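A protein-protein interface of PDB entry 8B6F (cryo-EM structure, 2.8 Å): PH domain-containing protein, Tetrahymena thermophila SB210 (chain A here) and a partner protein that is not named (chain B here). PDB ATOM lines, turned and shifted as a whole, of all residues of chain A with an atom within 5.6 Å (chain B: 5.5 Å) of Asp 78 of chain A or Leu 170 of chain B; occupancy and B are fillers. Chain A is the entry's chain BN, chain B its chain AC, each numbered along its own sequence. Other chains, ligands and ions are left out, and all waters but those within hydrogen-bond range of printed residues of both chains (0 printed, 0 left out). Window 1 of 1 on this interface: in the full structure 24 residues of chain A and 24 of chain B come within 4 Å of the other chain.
The side-chain amino group (NZ) of Lys 110 of chain B lies within hydrogen-bond range of the backbone carbonyl oxygen (O) of Ser 72 of chain A, 3.0 Å away. The backbone carbonyl oxygen (O) of His 75 of chain A lies within hydrogen-bond range of the side-chain amino group (NZ) of Lys 110 of chain B (3.1 Å). ND2 of Asn 167 of chain B is in hydrogen-bond range of OG1 of Thr 81 of chain A, at 2.9 Å. OH of Tyr 227 of chain B sits at hydrogen-bond distance from OG1 of Thr 77 of chain A (2.8 Å).
O of Tyr 227 of chain B sits close to OD1 of Asn 167 of chain B (3.2 Å). The backbone NH of Ile 168 of chain B lies within hydrogen-bond range of the backbone carbonyl oxygen of Tyr 227 of chain B (3.0 Å). The backbone carbonyl oxygen (O) of Leu 170 of chain B sits at hydrogen-bond distance from the side-chain sulfur (SG) of Cys 174 of chain B, at 3.2 Å. A ring nitrogen (ND1) of His 75 of chain A lies within hydrogen-bond range of the backbone NH (N) of Thr 77 of chain A, 3.1 Å away. OD1 of Asp 78 of chain A is in hydrogen-bond range of OG1 of Thr 81 of chain A. O of Val 80 of chain A sits at hydrogen-bond distance from OG of Ser 83 of chain A, 2.6 Å away.
Pro 76 of chain A touches Lys 110 of chain B (O to CD, 2.9 Å). Asp 78 of chain A touches Phe 109 of chain B (CB to O, 3.3 Å). Asp 78 of chain A touches Asn 167 of chain B. Asp 78 of chain A touches Leu 170 of chain B. Leu 169 of chain B touches Val 80 of chain A. CA of Thr 81 of chain A touches CD2 of Leu 169 of chain B (3.5 Å). CG of Tyr 227 of chain B touches CG2 of Thr 81 of chain A (3.5 Å).
Of the printed residues of chain B, Asp 78 of chain A touches Phe 109 (3.3 Å), Asn 167 (3.99 Å) and Leu 170 (3.3 Å). Of chain A, only Asp 78 (3.3 Å) comes within 4 Å of Leu 170 of chain B. Of the printed residues of chain A, Tyr 227 of chain B touches Thr 77 and Thr 81. Of the printed residues of chain B, Ser 72 of chain A touches Lys 110. Of the printed residues of chain A, Phe 109 of chain B touches Asp 78. Of the printed residues of chain B, Val 80 of chain A touches Leu 169 (3.2 Å). Printed residues of chain A within 4 Å of Leu 169 of chain B: Val 80 (3.2 Å) and Thr 81 (3.5 Å). The nearest residue of chain A that does not touch Leu 170 of chain B is Thr 81 of chain A (4.2 Å).
Hydrophobic or aromatic side chains of chain A that line the printed part of chain B: Val 80. Along chain A the printed residues that touch a printed residue of chain B span positions 72 to 81. Hydrophobic or aromatic side chains of chain B within 4 Å of the printed part of chain A: Leu 169, Leu 170 and Tyr 227. Among the printed residues, no Asp or Glu carboxylate lies within 4 Å of a Lys or Arg side-chain nitrogen of the other chain.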
ATOM      1  N   SER A  72     -22.727 -39.980 -13.033  1.00  0.00           N
ATOM      2  CA  SER A  72     -21.453 -39.968 -12.331  1.00  0.00           C
ATOM      3  C   SER A  72     -21.109 -41.299 -11.678  1.00  0.00           C
ATOM      4  O   SER A  72     -20.003 -41.436 -11.145  1.00  0.00           O
ATOM      5  CB  SER A  72     -21.455 -38.882 -11.261  1.00  0.00           C
ATOM      6  OG  SER A  72     -22.622 -38.974 -10.474  1.00  0.00           O
ATOM      7  N   HIS A  75     -17.486 -42.878 -11.737  1.00  0.00           N
ATOM      8  CA  HIS A  75     -16.331 -42.378 -11.002  1.00  0.00           C
ATOM      9  C   HIS A  75     -16.770 -41.581  -9.780  1.00  0.00           C
ATOM     10  O   HIS A  75     -17.749 -40.824  -9.859  1.00  0.00           O
ATOM     11  CB  HIS A  75     -15.471 -41.490 -11.901  1.00  0.00           C
ATOM     12  CG  HIS A  75     -14.052 -41.348 -11.444  1.00  0.00           C
ATOM     13  ND1 HIS A  75     -13.630 -40.311 -10.641  1.00  0.00           N
ATOM     14  CD2 HIS A  75     -12.958 -42.105 -11.684  1.00  0.00           C
ATOM     15  CE1 HIS A  75     -12.339 -40.441 -10.400  1.00  0.00           C
ATOM     16  NE2 HIS A  75     -11.906 -41.521 -11.023  1.00  0.00           N
ATOM     17  N   PRO A  76     -16.077 -41.720  -8.646  1.00  0.00           N
ATOM     18  CA  PRO A  76     -16.449 -40.913  -7.470  1.00  0.00           C
ATOM     19  C   PRO A  76     -16.325 -39.414  -7.685  1.00  0.00           C
ATOM     20  O   PRO A  76     -17.091 -38.648  -7.092  1.00  0.00           O
ATOM     21  CB  PRO A  76     -15.483 -41.408  -6.387  1.00  0.00           C
ATOM     22  CG  PRO A  76     -14.349 -42.017  -7.125  1.00  0.00           C
ATOM     23  CD  PRO A  76     -14.938 -42.608  -8.359  1.00  0.00           C
ATOM     24  N   THR A  77     -15.370 -38.966  -8.494  1.00  0.00           N
ATOM     25  CA  THR A  77     -15.238 -37.547  -8.789  1.00  0.00           C
ATOM     26  C   THR A  77     -16.359 -37.091  -9.719  1.00  0.00           C
ATOM     27  O   THR A  77     -16.886 -37.863 -10.522  1.00  0.00           O
ATOM     28  CB  THR A  77     -13.874 -37.268  -9.429  1.00  0.00           C
ATOM     29  OG1 THR A  77     -12.830 -37.698  -8.547  1.00  0.00           O
ATOM     30  CG2 THR A  77     -13.695 -35.788  -9.718  1.00  0.00           C
ATOM     31  N   ASP A  78     -16.723 -35.816  -9.602  1.00  0.00           N
ATOM     32  CA  ASP A  78     -17.791 -35.267 -10.422  1.00  0.00           C
ATOM     33  C   ASP A  78     -17.362 -35.183 -11.885  1.00  0.00           C
ATOM     34  O   ASP A  78     -16.174 -35.183 -12.218  1.00  0.00           O
ATOM     35  CB  ASP A  78     -18.208 -33.886  -9.918  1.00  0.00           C
ATOM     36  CG  ASP A  78     -17.030 -32.954  -9.730  1.00  0.00           C
ATOM     37  OD1 ASP A  78     -15.978 -33.417  -9.247  1.00  0.00           O
ATOM     38  OD2 ASP A  78     -17.158 -31.759 -10.065  1.00  0.00           O
ATOM     39  N   LYS A  79     -18.361 -35.111 -12.766  1.00  0.00           N
ATOM     40  CA  LYS A  79     -18.101 -35.182 -14.201  1.00  0.00           C
ATOM     41  C   LYS A  79     -17.318 -33.972 -14.694  1.00  0.00           C
ATOM     42  O   LYS A  79     -16.410 -34.110 -15.522  1.00  0.00           O
ATOM     43  CB  LYS A  79     -19.417 -35.308 -14.962  1.00  0.00           C
ATOM     44  CG  LYS A  79     -20.258 -36.495 -14.531  1.00  0.00           C
ATOM     45  CD  LYS A  79     -21.514 -36.632 -15.377  1.00  0.00           C
ATOM     46  CE  LYS A  79     -21.200 -37.087 -16.792  1.00  0.00           C
ATOM     47  NZ  LYS A  79     -20.535 -38.420 -16.808  1.00  0.00           N
ATOM     48  N   VAL A  80     -17.652 -32.780 -14.201  1.00  0.00           N
ATOM     49  CA  VAL A  80     -16.953 -31.573 -14.637  1.00  0.00           C
ATOM     50  C   VAL A  80     -15.485 -31.639 -14.239  1.00  0.00           C
ATOM     51  O   VAL A  80     -14.594 -31.309 -15.030  1.00  0.00           O
ATOM     52  CB  VAL A  80     -17.640 -30.319 -14.067  1.00  0.00           C
ATOM     53  CG1 VAL A  80     -16.944 -29.060 -14.558  1.00  0.00           C
ATOM     54  CG2 VAL A  80     -19.109 -30.293 -14.454  1.00  0.00           C
ATOM     55  N   THR A  81     -15.212 -32.063 -13.006  1.00  0.00           N
ATOM     56  CA  THR A  81     -13.832 -32.216 -12.561  1.00  0.00           C
ATOM     57  C   THR A  81     -13.103 -33.273 -13.380  1.00  0.00           C
ATOM     58  O   THR A  81     -11.936 -33.091 -13.744  1.00  0.00           O
ATOM     59  CB  THR A  81     -13.808 -32.578 -11.079  1.00  0.00           C
ATOM     60  OG1 THR A  81     -14.522 -31.585 -10.336  1.00  0.00           O
ATOM     61  CG2 THR A  81     -12.377 -32.664 -10.564  1.00  0.00           C
ATOM     62  N   LEU A  82     -13.775 -34.381 -13.689  1.00  0.00           N
ATOM     63  CA  LEU A  82     -13.162 -35.402 -14.530  1.00  0.00           C
ATOM     64  C   LEU A  82     -12.802 -34.852 -15.899  1.00  0.00           C
ATOM     65  O   LEU A  82     -11.721 -35.134 -16.427  1.00  0.00           O
ATOM     66  CB  LEU A  82     -14.106 -36.589 -14.686  1.00  0.00           C
ATOM     67  CG  LEU A  82     -14.127 -37.579 -13.532  1.00  0.00           C
ATOM     68  CD1 LEU A  82     -15.251 -38.547 -13.757  1.00  0.00           C
ATOM     69  CD2 LEU A  82     -12.802 -38.311 -13.409  1.00  0.00           C
ATOM     70  N   SER A  83     -13.695 -34.064 -16.493  1.00  0.00           N
ATOM     71  CA  SER A  83     -13.450 -33.564 -17.838  1.00  0.00           C
ATOM     72  C   SER A  83     -12.278 -32.591 -17.869  1.00  0.00           C
ATOM     73  O   SER A  83     -11.414 -32.684 -18.748  1.00  0.00           O
ATOM     74  CB  SER A  83     -14.717 -32.901 -18.382  1.00  0.00           C
ATOM     75  OG  SER A  83     -15.198 -31.912 -17.491  1.00  0.00           O
ATOM     76  N   PHE B 109     -22.617 -32.307  -6.714  1.00  0.00           N
ATOM     77  CA  PHE B 109     -21.364 -32.432  -7.457  1.00  0.00           C
ATOM     78  C   PHE B 109     -20.354 -33.310  -6.724  1.00  0.00           C
ATOM     79  O   PHE B 109     -19.143 -33.136  -6.876  1.00  0.00           O
ATOM     80  CB  PHE B 109     -20.760 -31.057  -7.753  1.00  0.00           C
ATOM     81  CG  PHE B 109     -21.658 -30.175  -8.558  1.00  0.00           C
ATOM     82  CD1 PHE B 109     -21.659 -30.244  -9.940  1.00  0.00           C
ATOM     83  CD2 PHE B 109     -22.511 -29.282  -7.935  1.00  0.00           C
ATOM     84  CE1 PHE B 109     -22.491 -29.437 -10.686  1.00  0.00           C
ATOM     85  CE2 PHE B 109     -23.346 -28.474  -8.672  1.00  0.00           C
ATOM     86  CZ  PHE B 109     -23.336 -28.550 -10.052  1.00  0.00           C
ATOM     87  N   LYS B 110     -20.844 -34.257  -5.926  1.00  0.00           N
ATOM     88  CA  LYS B 110     -19.991 -35.236  -5.253  1.00  0.00           C
ATOM     89  C   LYS B 110     -18.815 -34.562  -4.550  1.00  0.00           C
ATOM     90  O   LYS B 110     -17.682 -35.044  -4.589  1.00  0.00           O
ATOM     91  CB  LYS B 110     -19.493 -36.297  -6.235  1.00  0.00           C
ATOM     92  CG  LYS B 110     -20.574 -37.235  -6.741  1.00  0.00           C
ATOM     93  CD  LYS B 110     -19.962 -38.504  -7.312  1.00  0.00           C
ATOM     94  CE  LYS B 110     -21.027 -39.518  -7.679  1.00  0.00           C
ATOM     95  NZ  LYS B 110     -20.444 -40.765  -8.241  1.00  0.00           N
ATOM     96  N   SER B 111     -19.088 -33.439  -3.894  1.00  0.00           N
ATOM     97  CA  SER B 111     -18.063 -32.656  -3.220  1.00  0.00           C
ATOM     98  C   SER B 111     -18.428 -32.508  -1.751  1.00  0.00           C
ATOM     99  O   SER B 111     -19.584 -32.225  -1.421  1.00  0.00           O
ATOM    100  CB  SER B 111     -17.902 -31.279  -3.869  1.00  0.00           C
ATOM    101  OG  SER B 111     -19.093 -30.520  -3.766  1.00  0.00           O
ATOM    102  N   VAL B 161     -22.680 -22.690  -3.918  1.00  0.00           N
ATOM    103  CA  VAL B 161     -21.716 -23.688  -4.368  1.00  0.00           C
ATOM    104  C   VAL B 161     -20.316 -23.088  -4.393  1.00  0.00           C
ATOM    105  O   VAL B 161     -19.328 -23.778  -4.119  1.00  0.00           O
ATOM    106  CB  VAL B 161     -22.118 -24.249  -5.744  1.00  0.00           C
ATOM    107  CG1 VAL B 161     -21.149 -25.338  -6.182  1.00  0.00           C
ATOM    108  CG2 VAL B 161     -23.539 -24.789  -5.707  1.00  0.00           C
ATOM    109  N   TYR B 162     -20.212 -21.799  -4.725  1.00  0.00           N
ATOM    110  CA  TYR B 162     -18.913 -21.135  -4.796  1.00  0.00           C
ATOM    111  C   TYR B 162     -18.218 -21.118  -3.441  1.00  0.00           C
ATOM    112  O   TYR B 162     -17.005 -21.341  -3.357  1.00  0.00           O
ATOM    113  CB  TYR B 162     -19.111 -19.710  -5.319  1.00  0.00           C
ATOM    114  CG  TYR B 162     -17.845 -18.921  -5.572  1.00  0.00           C
ATOM    115  CD1 TYR B 162     -16.839 -19.417  -6.387  1.00  0.00           C
ATOM    116  CD2 TYR B 162     -17.682 -17.652  -5.033  1.00  0.00           C
ATOM    117  CE1 TYR B 162     -15.694 -18.684  -6.634  1.00  0.00           C
ATOM    118  CE2 TYR B 162     -16.542 -16.914  -5.273  1.00  0.00           C
ATOM    119  CZ  TYR B 162     -15.553 -17.435  -6.074  1.00  0.00           C
ATOM    120  OH  TYR B 162     -14.416 -16.702  -6.316  1.00  0.00           O
ATOM    121  N   VAL B 165     -17.410 -25.168  -1.354  1.00  0.00           N
ATOM    122  CA  VAL B 165     -16.742 -26.186  -2.155  1.00  0.00           C
ATOM    123  C   VAL B 165     -15.243 -26.088  -1.913  1.00  0.00           C
ATOM    124  O   VAL B 165     -14.699 -24.991  -1.753  1.00  0.00           O
ATOM    125  CB  VAL B 165     -17.075 -26.039  -3.656  1.00  0.00           C
ATOM    126  CG1 VAL B 165     -16.317 -24.868  -4.279  1.00  0.00           C
ATOM    127  CG2 VAL B 165     -16.772 -27.329  -4.392  1.00  0.00           C
ATOM    128  N   ASN B 167     -13.065 -27.553  -4.143  1.00  0.00           N
ATOM    129  CA  ASN B 167     -12.536 -27.980  -5.430  1.00  0.00           C
ATOM    130  C   ASN B 167     -12.161 -26.756  -6.253  1.00  0.00           C
ATOM    131  O   ASN B 167     -12.964 -25.828  -6.393  1.00  0.00           O
ATOM    132  CB  ASN B 167     -13.565 -28.835  -6.170  1.00  0.00           C
ATOM    133  CG  ASN B 167     -13.001 -29.471  -7.417  1.00  0.00           C
ATOM    134  OD1 ASN B 167     -12.097 -28.934  -8.052  1.00  0.00           O
ATOM    135  ND2 ASN B 167     -13.527 -30.631  -7.771  1.00  0.00           N
ATOM    136  N   ILE B 168     -10.940 -26.754  -6.787  1.00  0.00           N
ATOM    137  CA  ILE B 168     -10.463 -25.598  -7.541  1.00  0.00           C
ATOM    138  C   ILE B 168     -11.302 -25.394  -8.796  1.00  0.00           C
ATOM    139  O   ILE B 168     -11.702 -24.271  -9.121  1.00  0.00           O
ATOM    140  CB  ILE B 168      -8.972 -25.760  -7.888  1.00  0.00           C
ATOM    141  CG1 ILE B 168      -8.141 -25.892  -6.609  1.00  0.00           C
ATOM    142  CG2 ILE B 168      -8.487 -24.578  -8.721  1.00  0.00           C
ATOM    143  CD1 ILE B 168      -6.690 -26.250  -6.852  1.00  0.00           C
ATOM    144  N   LEU B 169     -11.581 -26.477  -9.523  1.00  0.00           N
ATOM    145  CA  LEU B 169     -12.323 -26.338 -10.771  1.00  0.00           C
ATOM    146  C   LEU B 169     -13.751 -25.876 -10.521  1.00  0.00           C
ATOM    147  O   LEU B 169     -14.251 -24.987 -11.219  1.00  0.00           O
ATOM    148  CB  LEU B 169     -12.319 -27.657 -11.537  1.00  0.00           C
ATOM    149  CG  LEU B 169     -12.928 -27.535 -12.935  1.00  0.00           C
ATOM    150  CD1 LEU B 169     -11.904 -26.998 -13.918  1.00  0.00           C
ATOM    151  CD2 LEU B 169     -13.461 -28.863 -13.387  1.00  0.00           C
ATOM    152  N   LEU B 170     -14.424 -26.461  -9.530  1.00  0.00           N
ATOM    153  CA  LEU B 170     -15.774 -26.016  -9.207  1.00  0.00           C
ATOM    154  C   LEU B 170     -15.760 -24.571  -8.738  1.00  0.00           C
ATOM    155  O   LEU B 170     -16.658 -23.789  -9.069  1.00  0.00           O
ATOM    156  CB  LEU B 170     -16.389 -26.922  -8.143  1.00  0.00           C
ATOM    157  CG  LEU B 170     -16.600 -28.383  -8.547  1.00  0.00           C
ATOM    158  CD1 LEU B 170     -17.126 -29.189  -7.373  1.00  0.00           C
ATOM    159  CD2 LEU B 170     -17.545 -28.491  -9.733  1.00  0.00           C
ATOM    160  N   PHE B 171     -14.745 -24.203  -7.958  1.00  0.00           N
ATOM    161  CA  PHE B 171     -14.582 -22.815  -7.547  1.00  0.00           C
ATOM    162  C   PHE B 171     -14.530 -21.894  -8.759  1.00  0.00           C
ATOM    163  O   PHE B 171     -15.263 -20.902  -8.835  1.00  0.00           O
ATOM    164  CB  PHE B 171     -13.310 -22.691  -6.709  1.00  0.00           C
ATOM    165  CG  PHE B 171     -13.189 -21.398  -5.975  1.00  0.00           C
ATOM    166  CD1 PHE B 171     -13.769 -21.242  -4.731  1.00  0.00           C
ATOM    167  CD2 PHE B 171     -12.470 -20.347  -6.512  1.00  0.00           C
ATOM    168  CE1 PHE B 171     -13.653 -20.057  -4.045  1.00  0.00           C
ATOM    169  CE2 PHE B 171     -12.349 -19.158  -5.832  1.00  0.00           C
ATOM    170  CZ  PHE B 171     -12.942 -19.011  -4.594  1.00  0.00           C
ATOM    171  N   PHE B 172     -13.667 -22.215  -9.724  1.00  0.00           N
ATOM    172  CA  PHE B 172     -13.520 -21.372 -10.906  1.00  0.00           C
ATOM    173  C   PHE B 172     -14.799 -21.339 -11.733  1.00  0.00           C
ATOM    174  O   PHE B 172     -15.196 -20.282 -12.233  1.00  0.00           O
ATOM    175  CB  PHE B 172     -12.345 -21.860 -11.752  1.00  0.00           C
ATOM    176  CG  PHE B 172     -12.181 -21.115 -13.042  1.00  0.00           C
ATOM    177  CD1 PHE B 172     -11.813 -19.780 -13.042  1.00  0.00           C
ATOM    178  CD2 PHE B 172     -12.375 -21.752 -14.255  1.00  0.00           C
ATOM    179  CE1 PHE B 172     -11.653 -19.092 -14.228  1.00  0.00           C
ATOM    180  CE2 PHE B 172     -12.218 -21.068 -15.446  1.00  0.00           C
ATOM    181  CZ  PHE B 172     -11.855 -19.736 -15.431  1.00  0.00           C
ATOM    182  N   MET B 173     -15.460 -22.488 -11.885  1.00  0.00           N
ATOM    183  CA  MET B 173     -16.688 -22.536 -12.673  1.00  0.00           C
ATOM    184  C   MET B 173     -17.791 -21.707 -12.031  1.00  0.00           C
ATOM    185  O   MET B 173     -18.514 -20.982 -12.723  1.00  0.00           O
ATOM    186  CB  MET B 173     -17.142 -23.984 -12.852  1.00  0.00           C
ATOM    187  CG  MET B 173     -16.224 -24.819 -13.734  1.00  0.00           C
ATOM    188  SD  MET B 173     -16.071 -24.182 -15.414  1.00  0.00           S
ATOM    189  CE  MET B 173     -17.766 -24.270 -15.982  1.00  0.00           C
ATOM    190  N   CYS B 174     -17.924 -21.780 -10.707  1.00  0.00           N
ATOM    191  CA  CYS B 174     -18.908 -20.946 -10.026  1.00  0.00           C
ATOM    192  C   CYS B 174     -18.586 -19.468 -10.198  1.00  0.00           C
ATOM    193  O   CYS B 174     -19.489 -18.647 -10.384  1.00  0.00           O
ATOM    194  CB  CYS B 174     -18.965 -21.306  -8.545  1.00  0.00           C
ATOM    195  SG  CYS B 174     -19.660 -22.919  -8.196  1.00  0.00           S
ATOM    196  N   TYR B 175     -17.303 -19.110 -10.135  1.00  0.00           N
ATOM    197  CA  TYR B 175     -16.919 -17.722 -10.360  1.00  0.00           C
ATOM    198  C   TYR B 175     -17.311 -17.265 -11.760  1.00  0.00           C
ATOM    199  O   TYR B 175     -17.778 -16.137 -11.944  1.00  0.00           O
ATOM    200  CB  TYR B 175     -15.415 -17.550 -10.148  1.00  0.00           C
ATOM    201  CG  TYR B 175     -14.906 -16.187 -10.555  1.00  0.00           C
ATOM    202  CD1 TYR B 175     -15.066 -15.089  -9.722  1.00  0.00           C
ATOM    203  CD2 TYR B 175     -14.266 -15.999 -11.772  1.00  0.00           C
ATOM    204  CE1 TYR B 175     -14.604 -13.841 -10.088  1.00  0.00           C
ATOM    205  CE2 TYR B 175     -13.801 -14.755 -12.148  1.00  0.00           C
ATOM    206  CZ  TYR B 175     -13.974 -13.679 -11.302  1.00  0.00           C
ATOM    207  OH  TYR B 175     -13.512 -12.438 -11.670  1.00  0.00           O
ATOM    208  N   TYR B 227      -6.939 -31.321  -7.717  1.00  0.00           N
ATOM    209  CA  TYR B 227      -8.036 -30.368  -7.708  1.00  0.00           C
ATOM    210  C   TYR B 227      -8.611 -30.137  -6.319  1.00  0.00           C
ATOM    211  O   TYR B 227      -9.580 -29.384  -6.195  1.00  0.00           O
ATOM    212  CB  TYR B 227      -9.162 -30.837  -8.645  1.00  0.00           C
ATOM    213  CG  TYR B 227      -9.819 -32.124  -8.203  1.00  0.00           C
ATOM    214  CD1 TYR B 227     -10.870 -32.112  -7.296  1.00  0.00           C
ATOM    215  CD2 TYR B 227      -9.389 -33.349  -8.692  1.00  0.00           C
ATOM    216  CE1 TYR B 227     -11.475 -33.279  -6.888  1.00  0.00           C
ATOM    217  CE2 TYR B 227      -9.988 -34.525  -8.289  1.00  0.00           C
ATOM    218  CZ  TYR B 227     -11.032 -34.482  -7.385  1.00  0.00           C
ATOM    219  OH  TYR B 227     -11.634 -35.648  -6.979  1.00  0.00           O
